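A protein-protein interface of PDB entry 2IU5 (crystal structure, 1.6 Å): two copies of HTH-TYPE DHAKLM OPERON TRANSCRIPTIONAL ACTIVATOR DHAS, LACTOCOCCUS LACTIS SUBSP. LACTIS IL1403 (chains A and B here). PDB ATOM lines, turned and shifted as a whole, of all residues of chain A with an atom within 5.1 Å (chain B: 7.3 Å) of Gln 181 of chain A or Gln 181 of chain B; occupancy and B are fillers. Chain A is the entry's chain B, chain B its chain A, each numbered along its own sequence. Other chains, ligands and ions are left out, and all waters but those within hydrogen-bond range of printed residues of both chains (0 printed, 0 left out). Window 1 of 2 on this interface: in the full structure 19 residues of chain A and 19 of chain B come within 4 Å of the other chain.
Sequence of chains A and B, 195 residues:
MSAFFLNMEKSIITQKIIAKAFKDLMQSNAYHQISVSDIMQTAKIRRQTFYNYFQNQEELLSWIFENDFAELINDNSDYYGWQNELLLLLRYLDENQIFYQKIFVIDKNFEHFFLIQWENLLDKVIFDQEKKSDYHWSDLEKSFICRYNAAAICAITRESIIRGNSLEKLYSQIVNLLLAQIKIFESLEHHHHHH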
ATOM      1  N   ILE A 145      31.115  -8.339  10.118  1.00  0.00           N
ATOM      2  CA  ILE A 145      29.976  -9.028   9.512  1.00  0.00           C
ATOM      3  C   ILE A 145      30.419 -10.348   8.900  1.00  0.00           C
ATOM      4  O   ILE A 145      29.752 -11.381   9.029  1.00  0.00           O
ATOM      5  CB  ILE A 145      29.346  -8.151   8.437  1.00  0.00           C
ATOM      6  CG1 ILE A 145      28.572  -7.032   9.134  1.00  0.00           C
ATOM      7  CG2 ILE A 145      28.449  -8.981   7.503  1.00  0.00           C
ATOM      8  CD1 ILE A 145      28.071  -5.977   8.140  1.00  0.00           C
ATOM      9  N   TYR A 148      31.545 -12.878  11.754  1.00  0.00           N
ATOM     10  CA  TYR A 148      30.366 -13.321  12.501  1.00  0.00           C
ATOM     11  C   TYR A 148      29.554 -14.321  11.701  1.00  0.00           C
ATOM     12  O   TYR A 148      29.209 -15.383  12.191  1.00  0.00           O
ATOM     13  CB  TYR A 148      29.520 -12.095  12.805  1.00  0.00           C
ATOM     14  CG  TYR A 148      28.312 -12.265  13.712  1.00  0.00           C
ATOM     15  CD1 TYR A 148      28.429 -11.982  15.069  1.00  0.00           C
ATOM     16  CD2 TYR A 148      27.075 -12.684  13.216  1.00  0.00           C
ATOM     17  CE1 TYR A 148      27.351 -12.121  15.917  1.00  0.00           C
ATOM     18  CE2 TYR A 148      25.972 -12.833  14.056  1.00  0.00           C
ATOM     19  CZ  TYR A 148      26.124 -12.546  15.404  1.00  0.00           C
ATOM     20  OH  TYR A 148      25.044 -12.678  16.257  1.00  0.00           O
ATOM     21  N   ASN A 149      29.246 -13.967  10.457  1.00  0.00           N
ATOM     22  CA  ASN A 149      28.390 -14.818   9.649  1.00  0.00           C
ATOM     23  C   ASN A 149      29.083 -16.059   9.128  1.00  0.00           C
ATOM     24  O   ASN A 149      28.447 -17.107   8.981  1.00  0.00           O
ATOM     25  CB  ASN A 149      27.733 -13.983   8.566  1.00  0.00           C
ATOM     26  CG  ASN A 149      26.654 -13.099   9.162  1.00  0.00           C
ATOM     27  OD1 ASN A 149      25.550 -13.575   9.442  1.00  0.00           O
ATOM     28  ND2 ASN A 149      26.968 -11.814   9.368  1.00  0.00           N
ATOM     29  N   LEU A 177      18.649 -13.825   6.818  1.00  0.00           N
ATOM     30  CA  LEU A 177      19.407 -13.243   7.932  1.00  0.00           C
ATOM     31  C   LEU A 177      20.584 -12.399   7.457  1.00  0.00           C
ATOM     32  O   LEU A 177      20.896 -11.333   8.040  1.00  0.00           O
ATOM     33  CB  LEU A 177      19.899 -14.321   8.915  1.00  0.00           C
ATOM     34  CG  LEU A 177      18.845 -15.192   9.604  1.00  0.00           C
ATOM     35  CD1 LEU A 177      19.487 -16.181  10.597  1.00  0.00           C
ATOM     36  CD2 LEU A 177      17.766 -14.371  10.303  1.00  0.00           C
ATOM     37  N   LEU A 178      21.254 -12.858   6.401  1.00  0.00           N
ATOM     38  CA  LEU A 178      22.344 -12.052   5.849  1.00  0.00           C
ATOM     39  C   LEU A 178      21.883 -10.732   5.241  1.00  0.00           C
ATOM     40  O   LEU A 178      22.483  -9.690   5.516  1.00  0.00           O
ATOM     41  CB  LEU A 178      23.107 -12.837   4.788  1.00  0.00           C
ATOM     42  CG  LEU A 178      23.957 -14.027   5.201  1.00  0.00           C
ATOM     43  CD1 LEU A 178      24.460 -14.693   3.919  1.00  0.00           C
ATOM     44  CD2 LEU A 178      25.138 -13.561   6.043  1.00  0.00           C
ATOM     45  N   LEU A 179      20.837 -10.777   4.430  1.00  0.00           N
ATOM     46  CA  LEU A 179      20.332  -9.577   3.769  1.00  0.00           C
ATOM     47  C   LEU A 179      19.888  -8.598   4.854  1.00  0.00           C
ATOM     48  O   LEU A 179      20.060  -7.401   4.706  1.00  0.00           O
ATOM     49  CB  LEU A 179      19.162  -9.915   2.839  1.00  0.00           C
ATOM     50  CG  LEU A 179      19.604 -10.615   1.551  1.00  0.00           C
ATOM     51  CD1 LEU A 179      18.404 -10.971   0.695  1.00  0.00           C
ATOM     52  CD2 LEU A 179      20.565  -9.708   0.817  1.00  0.00           C
ATOM     53  N   ALA A 180      19.323  -9.118   5.948  1.00  0.00           N
ATOM     54  CA  ALA A 180      18.816  -8.229   7.007  1.00  0.00           C
ATOM     55  C   ALA A 180      19.928  -7.428   7.669  1.00  0.00           C
ATOM     56  O   ALA A 180      19.784  -6.229   7.966  1.00  0.00           O
ATOM     57  CB  ALA A 180      18.097  -9.035   8.076  1.00  0.00           C
ATOM     58  N   GLN A 181      21.050  -8.099   7.909  1.00  0.00           N
ATOM     59  CA  GLN A 181      22.243  -7.457   8.436  1.00  0.00           C
ATOM     60  C   GLN A 181      22.860  -6.453   7.488  1.00  0.00           C
ATOM     61  O   GLN A 181      23.247  -5.372   7.906  1.00  0.00           O
ATOM     62  CB  GLN A 181      23.281  -8.505   8.833  1.00  0.00           C
ATOM     63  CG  GLN A 181      22.768  -9.454   9.893  1.00  0.00           C
ATOM     64  CD  GLN A 181      23.754 -10.565  10.153  1.00  0.00           C
ATOM     65  OE1 GLN A 181      24.869 -10.324  10.619  1.00  0.00           O
ATOM     66  NE2 GLN A 181      23.341 -11.797   9.844  1.00  0.00           N
ATOM     67  N   ILE A 182      22.959  -6.802   6.213  1.00  0.00           N
ATOM     68  CA  ILE A 182      23.611  -5.914   5.269  1.00  0.00           C
ATOM     69  C   ILE A 182      22.743  -4.677   5.057  1.00  0.00           C
ATOM     70  O   ILE A 182      23.260  -3.567   4.901  1.00  0.00           O
ATOM     71  CB  ILE A 182      23.846  -6.671   3.976  1.00  0.00           C
ATOM     72  CG1 ILE A 182      24.919  -7.728   4.249  1.00  0.00           C
ATOM     73  CG2 ILE A 182      24.265  -5.713   2.870  1.00  0.00           C
ATOM     74  CD1 ILE A 182      24.896  -8.865   3.246  1.00  0.00           C
ATOM     75  N   LYS A 183      21.429  -4.863   5.061  1.00  0.00           N
ATOM     76  CA  LYS A 183      20.508  -3.756   4.766  1.00  0.00           C
ATOM     77  C   LYS A 183      20.711  -2.583   5.727  1.00  0.00           C
ATOM     78  O   LYS A 183      20.517  -1.419   5.364  1.00  0.00           O
ATOM     79  CB  LYS A 183      19.051  -4.226   4.836  1.00  0.00           C
ATOM     80  CG  LYS A 183      18.014  -3.215   4.294  1.00  0.00           C
ATOM     81  CD  LYS A 183      16.746  -3.217   5.153  1.00  0.00           C
ATOM     82  CE  LYS A 183      15.582  -2.460   4.502  1.00  0.00           C
ATOM     83  NZ  LYS A 183      14.779  -1.650   5.477  1.00  0.00           N
ATOM     84  N   ILE A 184      21.099  -2.856   6.964  1.00  0.00           N
ATOM     85  CA  ILE A 184      21.248  -1.748   7.902  1.00  0.00           C
ATOM     86  C   ILE A 184      22.410  -0.816   7.577  1.00  0.00           C
ATOM     87  O   ILE A 184      22.460   0.314   8.083  1.00  0.00           O
ATOM     88  CB  ILE A 184      21.248  -2.175   9.387  1.00  0.00           C
ATOM     89  CG1 ILE A 184      22.571  -2.831   9.783  1.00  0.00           C
ATOM     90  CG2 ILE A 184      20.040  -3.032   9.705  1.00  0.00           C
ATOM     91  CD1 ILE A 184      22.644  -3.118  11.256  1.00  0.00           C
ATOM     92  N   PHE A 185      23.336  -1.274   6.742  1.00  0.00           N
ATOM     93  CA  PHE A 185      24.444  -0.419   6.318  1.00  0.00           C
ATOM     94  C   PHE A 185      24.243   0.279   4.977  1.00  0.00           C
ATOM     95  O   PHE A 185      25.081   1.061   4.555  1.00  0.00           O
ATOM     96  CB  PHE A 185      25.769  -1.179   6.350  1.00  0.00           C
ATOM     97  CG  PHE A 185      26.108  -1.709   7.710  1.00  0.00           C
ATOM     98  CD1 PHE A 185      25.755  -3.006   8.067  1.00  0.00           C
ATOM     99  CD2 PHE A 185      26.772  -0.910   8.626  1.00  0.00           C
ATOM    100  CE1 PHE A 185      26.062  -3.499   9.323  1.00  0.00           C
ATOM    101  CE2 PHE A 185      27.080  -1.411   9.888  1.00  0.00           C
ATOM    102  CZ  PHE A 185      26.719  -2.705  10.223  1.00  0.00           C
ATOM    103  N   TYR B 135       5.519 -11.279  16.212  1.00  0.00           N
ATOM    104  CA  TYR B 135       6.434 -11.859  15.208  1.00  0.00           C
ATOM    105  C   TYR B 135       5.742 -13.012  14.494  1.00  0.00           C
ATOM    106  O   TYR B 135       4.879 -13.658  15.088  1.00  0.00           O
ATOM    107  CB  TYR B 135       7.691 -12.372  15.914  1.00  0.00           C
ATOM    108  CG  TYR B 135       8.446 -11.214  16.491  1.00  0.00           C
ATOM    109  CD1 TYR B 135       9.401 -10.555  15.736  1.00  0.00           C
ATOM    110  CD2 TYR B 135       8.200 -10.767  17.784  1.00  0.00           C
ATOM    111  CE1 TYR B 135      10.094  -9.491  16.249  1.00  0.00           C
ATOM    112  CE2 TYR B 135       8.892  -9.698  18.308  1.00  0.00           C
ATOM    113  CZ  TYR B 135       9.839  -9.065  17.527  1.00  0.00           C
ATOM    114  OH  TYR B 135      10.557  -7.994  18.002  1.00  0.00           O
ATOM    115  N   TRP B 137       7.552 -15.505  13.102  1.00  0.00           N
ATOM    116  CA  TRP B 137       8.519 -16.604  13.076  1.00  0.00           C
ATOM    117  C   TRP B 137       7.903 -17.926  13.476  1.00  0.00           C
ATOM    118  O   TRP B 137       7.208 -18.009  14.479  1.00  0.00           O
ATOM    119  CB  TRP B 137       9.783 -16.343  13.907  1.00  0.00           C
ATOM    120  CG  TRP B 137       9.654 -15.705  15.279  1.00  0.00           C
ATOM    121  CD1 TRP B 137       8.654 -15.876  16.208  1.00  0.00           C
ATOM    122  CD2 TRP B 137      10.586 -14.792  15.862  1.00  0.00           C
ATOM    123  NE1 TRP B 137       8.919 -15.114  17.328  1.00  0.00           N
ATOM    124  CE2 TRP B 137      10.099 -14.441  17.139  1.00  0.00           C
ATOM    125  CE3 TRP B 137      11.788 -14.231  15.421  1.00  0.00           C
ATOM    126  CZ2 TRP B 137      10.778 -13.552  17.977  1.00  0.00           C
ATOM    127  CZ3 TRP B 137      12.465 -13.351  16.251  1.00  0.00           C
ATOM    128  CH2 TRP B 137      11.957 -13.019  17.523  1.00  0.00           C
ATOM    129  N   PHE B 144      16.247 -21.674  14.421  1.00  0.00           N
ATOM    130  CA  PHE B 144      17.366 -21.373  13.533  1.00  0.00           C
ATOM    131  C   PHE B 144      18.048 -20.074  13.922  1.00  0.00           C
ATOM    132  O   PHE B 144      19.278 -20.014  14.012  1.00  0.00           O
ATOM    133  CB  PHE B 144      16.903 -21.286  12.087  1.00  0.00           C
ATOM    134  CG  PHE B 144      18.030 -21.145  11.108  1.00  0.00           C
ATOM    135  CD1 PHE B 144      18.694 -22.263  10.628  1.00  0.00           C
ATOM    136  CD2 PHE B 144      18.422 -19.892  10.674  1.00  0.00           C
ATOM    137  CE1 PHE B 144      19.737 -22.136   9.723  1.00  0.00           C
ATOM    138  CE2 PHE B 144      19.472 -19.762   9.760  1.00  0.00           C
ATOM    139  CZ  PHE B 144      20.116 -20.888   9.296  1.00  0.00           C
ATOM    140  N   ILE B 145      17.268 -19.024  14.156  1.00  0.00           N
ATOM    141  CA  ILE B 145      17.864 -17.728  14.505  1.00  0.00           C
ATOM    142  C   ILE B 145      18.700 -17.865  15.784  1.00  0.00           C
ATOM    143  O   ILE B 145      19.804 -17.297  15.925  1.00  0.00           O
ATOM    144  CB  ILE B 145      16.789 -16.618  14.637  1.00  0.00           C
ATOM    145  CG1 ILE B 145      17.474 -15.287  14.969  1.00  0.00           C
ATOM    146  CG2 ILE B 145      15.846 -16.937  15.754  1.00  0.00           C
ATOM    147  CD1 ILE B 145      16.658 -14.094  14.521  1.00  0.00           C
ATOM    148  N   CYS B 146      18.187 -18.629  16.744  1.00  0.00           N
ATOM    149  CA  CYS B 146      18.935 -18.816  17.985  1.00  0.00           C
ATOM    150  C   CYS B 146      20.234 -19.583  17.771  1.00  0.00           C
ATOM    151  O   CYS B 146      21.290 -19.182  18.261  1.00  0.00           O
ATOM    152  CB  CYS B 146      18.072 -19.558  19.010  1.00  0.00           C
ATOM    153  SG  CYS B 146      16.695 -18.530  19.612  1.00  0.00           S
ATOM    154  N   TYR B 148      21.898 -20.089  14.998  1.00  0.00           N
ATOM    155  CA  TYR B 148      22.787 -19.341  14.095  1.00  0.00           C
ATOM    156  C   TYR B 148      23.566 -18.297  14.873  1.00  0.00           C
ATOM    157  O   TYR B 148      24.800 -18.257  14.828  1.00  0.00           O
ATOM    158  CB  TYR B 148      21.940 -18.658  13.026  1.00  0.00           C
ATOM    159  CG  TYR B 148      22.653 -17.949  11.872  1.00  0.00           C
ATOM    160  CD1 TYR B 148      22.873 -18.603  10.667  1.00  0.00           C
ATOM    161  CD2 TYR B 148      23.075 -16.636  12.004  1.00  0.00           C
ATOM    162  CE1 TYR B 148      23.510 -17.959   9.619  1.00  0.00           C
ATOM    163  CE2 TYR B 148      23.720 -15.963  10.964  1.00  0.00           C
ATOM    164  CZ  TYR B 148      23.924 -16.645   9.778  1.00  0.00           C
ATOM    165  OH  TYR B 148      24.557 -16.017   8.724  1.00  0.00           O
ATOM    166  N   ASN B 149      22.855 -17.433  15.587  1.00  0.00           N
ATOM    167  CA  ASN B 149      23.511 -16.388  16.351  1.00  0.00           C
ATOM    168  C   ASN B 149      24.311 -16.867  17.555  1.00  0.00           C
ATOM    169  O   ASN B 149      25.369 -16.304  17.849  1.00  0.00           O
ATOM    170  CB  ASN B 149      22.494 -15.299  16.677  1.00  0.00           C
ATOM    171  CG  ASN B 149      22.121 -14.533  15.438  1.00  0.00           C
ATOM    172  OD1 ASN B 149      22.892 -13.688  15.003  1.00  0.00           O
ATOM    173  ND2 ASN B 149      20.963 -14.822  14.862  1.00  0.00           N
ATOM    174  N   GLN B 173      28.098  -3.663  17.826  1.00  0.00           N
ATOM    175  CA  GLN B 173      27.936  -4.392  16.563  1.00  0.00           C
ATOM    176  C   GLN B 173      27.071  -5.640  16.745  1.00  0.00           C
ATOM    177  O   GLN B 173      26.239  -5.951  15.888  1.00  0.00           O
ATOM    178  CB  GLN B 173      29.306  -4.763  15.991  1.00  0.00           C
ATOM    179  CG  GLN B 173      30.074  -3.553  15.475  1.00  0.00           C
ATOM    180  CD  GLN B 173      31.471  -3.916  15.040  1.00  0.00           C
ATOM    181  OE1 GLN B 173      31.701  -4.207  13.860  1.00  0.00           O
ATOM    182  NE2 GLN B 173      32.407  -3.905  15.981  1.00  0.00           N
ATOM    183  N   ILE B 174      27.250  -6.362  17.848  1.00  0.00           N
ATOM    184  CA  ILE B 174      26.460  -7.554  18.059  1.00  0.00           C
ATOM    185  C   ILE B 174      24.992  -7.185  18.222  1.00  0.00           C
ATOM    186  O   ILE B 174      24.138  -7.794  17.591  1.00  0.00           O
ATOM    187  CB  ILE B 174      26.969  -8.411  19.234  1.00  0.00           C
ATOM    188  CG1 ILE B 174      28.376  -8.938  18.897  1.00  0.00           C
ATOM    189  CG2 ILE B 174      25.967  -9.539  19.524  1.00  0.00           C
ATOM    190  CD1 ILE B 174      29.157  -9.428  20.129  1.00  0.00           C
ATOM    191  N   VAL B 175      24.697  -6.191  19.062  1.00  0.00           N
ATOM    192  CA  VAL B 175      23.305  -5.765  19.253  1.00  0.00           C
ATOM    193  C   VAL B 175      22.662  -5.364  17.922  1.00  0.00           C
ATOM    194  O   VAL B 175      21.523  -5.735  17.623  1.00  0.00           O
ATOM    195  CB  VAL B 175      23.232  -4.614  20.280  1.00  0.00           C
ATOM    196  CG1 VAL B 175      21.811  -4.044  20.366  1.00  0.00           C
ATOM    197  CG2 VAL B 175      23.689  -5.122  21.628  1.00  0.00           C
ATOM    198  N   ASN B 176      23.389  -4.604  17.116  1.00  0.00           N
ATOM    199  CA  ASN B 176      22.823  -4.115  15.866  1.00  0.00           C
ATOM    200  C   ASN B 176      22.524  -5.261  14.901  1.00  0.00           C
ATOM    201  O   ASN B 176      21.479  -5.275  14.245  1.00  0.00           O
ATOM    202  CB  ASN B 176      23.736  -3.056  15.255  1.00  0.00           C
ATOM    203  CG  ASN B 176      23.786  -1.795  16.095  1.00  0.00           C
ATOM    204  OD1 ASN B 176      24.724  -1.001  15.988  1.00  0.00           O
ATOM    205  ND2 ASN B 176      22.771  -1.599  16.940  1.00  0.00           N
ATOM    206  N   LEU B 177      23.428  -6.233  14.815  1.00  0.00           N
ATOM    207  CA  LEU B 177      23.196  -7.357  13.924  1.00  0.00           C
ATOM    208  C   LEU B 177      22.008  -8.190  14.422  1.00  0.00           C
ATOM    209  O   LEU B 177      21.219  -8.715  13.631  1.00  0.00           O
ATOM    210  CB  LEU B 177      24.454  -8.205  13.796  1.00  0.00           C
ATOM    211  CG  LEU B 177      25.700  -7.539  13.194  1.00  0.00           C
ATOM    212  CD1 LEU B 177      26.790  -8.618  13.126  1.00  0.00           C
ATOM    213  CD2 LEU B 177      25.458  -6.991  11.800  1.00  0.00           C
ATOM    214  N   LEU B 178      21.876  -8.315  15.740  1.00  0.00           N
ATOM    215  CA  LEU B 178      20.784  -9.150  16.267  1.00  0.00           C
ATOM    216  C   LEU B 178      19.457  -8.453  16.011  1.00  0.00           C
ATOM    217  O   LEU B 178      18.502  -9.074  15.550  1.00  0.00           O
ATOM    218  CB  LEU B 178      20.946  -9.381  17.772  1.00  0.00           C
ATOM    219  CG  LEU B 178      22.070 -10.331  18.194  1.00  0.00           C
ATOM    220  CD1 LEU B 178      22.231 -10.299  19.723  1.00  0.00           C
ATOM    221  CD2 LEU B 178      21.833 -11.769  17.694  1.00  0.00           C
ATOM    222  N   LEU B 179      19.396  -7.160  16.312  1.00  0.00           N
ATOM    223  CA  LEU B 179      18.142  -6.426  16.095  1.00  0.00           C
ATOM    224  C   LEU B 179      17.738  -6.426  14.618  1.00  0.00           C
ATOM    225  O   LEU B 179      16.549  -6.495  14.303  1.00  0.00           O
ATOM    226  CB  LEU B 179      18.268  -4.987  16.596  1.00  0.00           C
ATOM    227  CG  LEU B 179      18.309  -4.833  18.121  1.00  0.00           C
ATOM    228  CD1 LEU B 179      18.766  -3.433  18.503  1.00  0.00           C
ATOM    229  CD2 LEU B 179      16.935  -5.109  18.707  1.00  0.00           C
ATOM    230  N   ALA B 180      18.708  -6.344  13.705  1.00  0.00           N
ATOM    231  CA  ALA B 180      18.380  -6.321  12.285  1.00  0.00           C
ATOM    232  C   ALA B 180      17.694  -7.611  11.863  1.00  0.00           C
ATOM    233  O   ALA B 180      16.754  -7.598  11.059  1.00  0.00           O
ATOM    234  CB  ALA B 180      19.642  -6.133  11.483  1.00  0.00           C
ATOM    235  N   GLN B 181      18.183  -8.712  12.418  1.00  0.00           N
ATOM    236  CA  GLN B 181      17.673 -10.030  12.061  1.00  0.00           C
ATOM    237  C   GLN B 181      16.296 -10.212  12.666  1.00  0.00           C
ATOM    238  O   GLN B 181      15.384 -10.727  12.007  1.00  0.00           O
ATOM    239  CB  GLN B 181      18.609 -11.068  12.646  1.00  0.00           C
ATOM    240  CG  GLN B 181      19.889 -11.191  11.868  1.00  0.00           C
ATOM    241  CD  GLN B 181      20.765 -12.206  12.531  1.00  0.00           C
ATOM    242  OE1 GLN B 181      20.508 -13.392  12.433  1.00  0.00           O
ATOM    243  NE2 GLN B 181      21.799 -11.749  13.213  1.00  0.00           N
ATOM    244  N   ILE B 182      16.142  -9.792  13.925  1.00  0.00           N
ATOM    245  CA  ILE B 182      14.852  -9.932  14.621  1.00  0.00           C
ATOM    246  C   ILE B 182      13.764  -9.175  13.853  1.00  0.00           C
ATOM    247  O   ILE B 182      12.617  -9.624  13.753  1.00  0.00           O
ATOM    248  CB  ILE B 182      14.959  -9.378  16.057  1.00  0.00           C
ATOM    249  CG1 ILE B 182      15.784 -10.324  16.919  1.00  0.00           C
ATOM    250  CG2 ILE B 182      13.578  -9.090  16.688  1.00  0.00           C
ATOM    251  CD1 ILE B 182      16.334  -9.676  18.183  1.00  0.00           C
ATOM    252  N   LYS B 183      14.134  -8.017  13.314  1.00  0.00           N
ATOM    253  CA  LYS B 183      13.165  -7.089  12.727  1.00  0.00           C
ATOM    254  C   LYS B 183      12.443  -7.679  11.521  1.00  0.00           C
ATOM    255  O   LYS B 183      11.270  -7.370  11.291  1.00  0.00           O
ATOM    256  CB  LYS B 183      13.833  -5.754  12.370  1.00  0.00           C
ATOM    257  CG  LYS B 183      12.850  -4.650  11.944  1.00  0.00           C
ATOM    258  CD  LYS B 183      12.547  -3.765  13.145  1.00  0.00           C
ATOM    259  CE  LYS B 183      12.443  -2.290  12.761  1.00  0.00           C
ATOM    260  NZ  LYS B 183      12.723  -1.394  13.932  1.00  0.00           N
ATOM    261  N   ILE B 184      13.117  -8.521  10.746  1.00  0.00           N
ATOM    262  CA  ILE B 184      12.459  -9.020   9.534  1.00  0.00           C
ATOM    263  C   ILE B 184      11.333  -9.997   9.836  1.00  0.00           C
ATOM    264  O   ILE B 184      10.537 -10.347   8.947  1.00  0.00           O
ATOM    265  CB  ILE B 184      13.453  -9.650   8.568  1.00  0.00           C
ATOM    266  CG1 ILE B 184      13.949 -10.983   9.133  1.00  0.00           C
ATOM    267  CG2 ILE B 184      14.569  -8.674   8.292  1.00  0.00           C
ATOM    268  CD1 ILE B 184      14.754 -11.814   8.149  1.00  0.00           C
ATOM    269  N   PHE B 185      11.243 -10.440  11.089  1.00  0.00           N
ATOM    270  CA  PHE B 185      10.173 -11.340  11.481  1.00  0.00           C
ATOM    271  C   PHE B 185       9.000 -10.629  12.150  1.00  0.00           C
ATOM    272  O   PHE B 185       8.038 -11.283  12.556  1.00  0.00           O
ATOM    273  CB  PHE B 185      10.693 -12.434  12.404  1.00  0.00           C
ATOM    274  CG  PHE B 185      11.713 -13.321  11.756  1.00  0.00           C
ATOM    275  CD1 PHE B 185      11.307 -14.398  10.989  1.00  0.00           C
ATOM    276  CD2 PHE B 185      13.068 -13.069  11.915  1.00  0.00           C
ATOM    277  CE1 PHE B 185      12.246 -15.223  10.386  1.00  0.00           C
ATOM    278  CE2 PHE B 185      14.009 -13.888  11.318  1.00  0.00           C
ATOM    279  CZ  PHE B 185      13.587 -14.963  10.555  1.00  0.00           C
ATOM    280  N   GLU B 186       9.082  -9.309  12.261  1.00  0.00           N
ATOM    281  CA  GLU B 186       7.895  -8.480  12.445  1.00  0.00           C
ATOM    282  C   GLU B 186       7.219  -8.475  11.086  1.00  0.00           C
ATOM    283  O   GLU B 186       6.418  -8.736  10.209  1.00  0.00           O
ATOM    284  CB  GLU B 186       8.269  -7.025  12.708  1.00  0.00           C
ATOM    285  CG  GLU B 186       8.882  -6.714  14.029  1.00  0.00           C
ATOM    286  CD  GLU B 186       9.157  -5.227  14.151  1.00  0.00           C
ATOM    287  OE1 GLU B 186       9.786  -4.810  15.142  1.00  0.00           O
ATOM    288  OE2 GLU B 186       8.739  -4.473  13.241  1.00  0.00           O
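Of chain A, only Leu 177 and Gln 181 come within 4 Å of Gln 181 of chain B.
Ala 180 of chain A touches two residues of chain B.
Printed residues of chain A within 4 Å of Ala 180 of chain B: Ala 180 and Ile 184.
Of the printed residues of chain B, Leu 178 of chain A touches Tyr 148.
Of the printed residues of chain B, Ile 184 of chain A touches Asn 176 (3.9 Å) and Ala 180 (3.6 Å).
Printed residues of chain A within 4 Å of Ile 184 of chain B: Ala 180.
Of the printed residues of chain A, Tyr 148 of chain B touches Asn 149 (2.7 Å), Leu 177 (3.8 Å) and Leu 178 (3.7 Å).
Ile 174 of chain B touches none of the printed residues of chain A.
The nearest residue of chain A that does not touch Gln 181 of chain B is Ala 180 of chain A (4.1 Å).
The nearest printed residue of chain A that does not touch Ala 180 of chain B is Gln 181 of chain A (4.2 Å).
Tyr 148 of chain A touches Leu 177 of chain B, and with the chains exchanged Leu 177 of chain A touches Tyr 148 of chain B.
Tyr 148 of chain A touches Leu 178 of chain B, and with the chains exchanged Leu 178 of chain A touches Tyr 148 of chain B.
Ala 180 of chain A touches its own counterpart, Ala 180 of chain B.
Gln 181 of chain A touches its own counterpart, Gln 181 of chain B.
Positions printed for both chains: 145, 148, 149, 177, 178, 179, 180, 181, 182, 183, 184 and 185.
Of the 15 pairs that touch across the chains among the printed residues, 12 have their exchanged pair printed and touching as well.
O of Leu 177 of chain B is in hydrogen-bond range of NE2 of Gln 181 of chain B, 3.1 Å away.
OE1 of Gln 181 of chain A is in hydrogen-bond range of ND2 of Asn 149 of chain A (2.9 Å).
The side-chain amide nitrogen (NE2) of Gln 181 of chain A is in hydrogen-bond range of the backbone carbonyl oxygen (O) of Leu 177 of chain A (3.1 Å).
The side-chain amide nitrogen of Asn 149 of chain B is in hydrogen-bond range of the side-chain amide oxygen of Gln 181 of chain B (2.9 Å).
The backbone carbonyl oxygen (O) of Ile 145 of chain B sits at hydrogen-bond distance from the side-chain amide nitrogen (ND2) of Asn 149 of chain B (2.9 Å).
The backbone carbonyl oxygen of Ile 145 of chain A is in hydrogen-bond range of the side-chain amide nitrogen of Asn 149 of chain A (2.8 Å).
Tyr 148 of chain A touches Leu 178 of chain B (OH to CD2, 3.6 Å).
CD1 of Leu 177 of chain A touches CE2 of Phe 144 of chain B (3.7 Å).
Leu 177 of chain A touches Tyr 148 of chain B (CD1 to CG, 3.8 Å).
Leu 177 of chain A touches Gln 181 of chain B.
CD2 of Leu 178 of chain A touches OH of Tyr 148 of chain B (3.7 Å).
Ala 180 of chain B touches Ala 180 of chain A (CB to O, 3.5 Å).
Ala 180 of chain A touches Ile 184 of chain B (CB to CG2, 3.6 Å).
CD2 of Leu 177 of chain B touches OE1 of Gln 181 of chain A, at 3.6 Å.
NE2 of Gln 181 of chain B touches NE2 of Gln 181 of chain A, 3.7 Å away.
Asn 176 of chain B touches Ile 184 of chain A (O to CD1, 3.9 Å).
Hydrophobic or aromatic side chains of chain B within 4 Å of the printed part of chain A: Phe 144, Tyr 148, Leu 177, Leu 178, Ala 180, Ile 184 and Phe 185.
Of the 12 printed residues of chain A, 7 touch a printed residue of chain B.
Among the printed residues, 15 pairs touch across the chains.
OH of Tyr 148 of chain A is in hydrogen-bond range of OD1 of Asn 149 of chain B, 2.7 Å away.
OH of Tyr 148 of chain B lies within hydrogen-bond range of OD1 of Asn 149 of chain A, 2.7 Å away.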
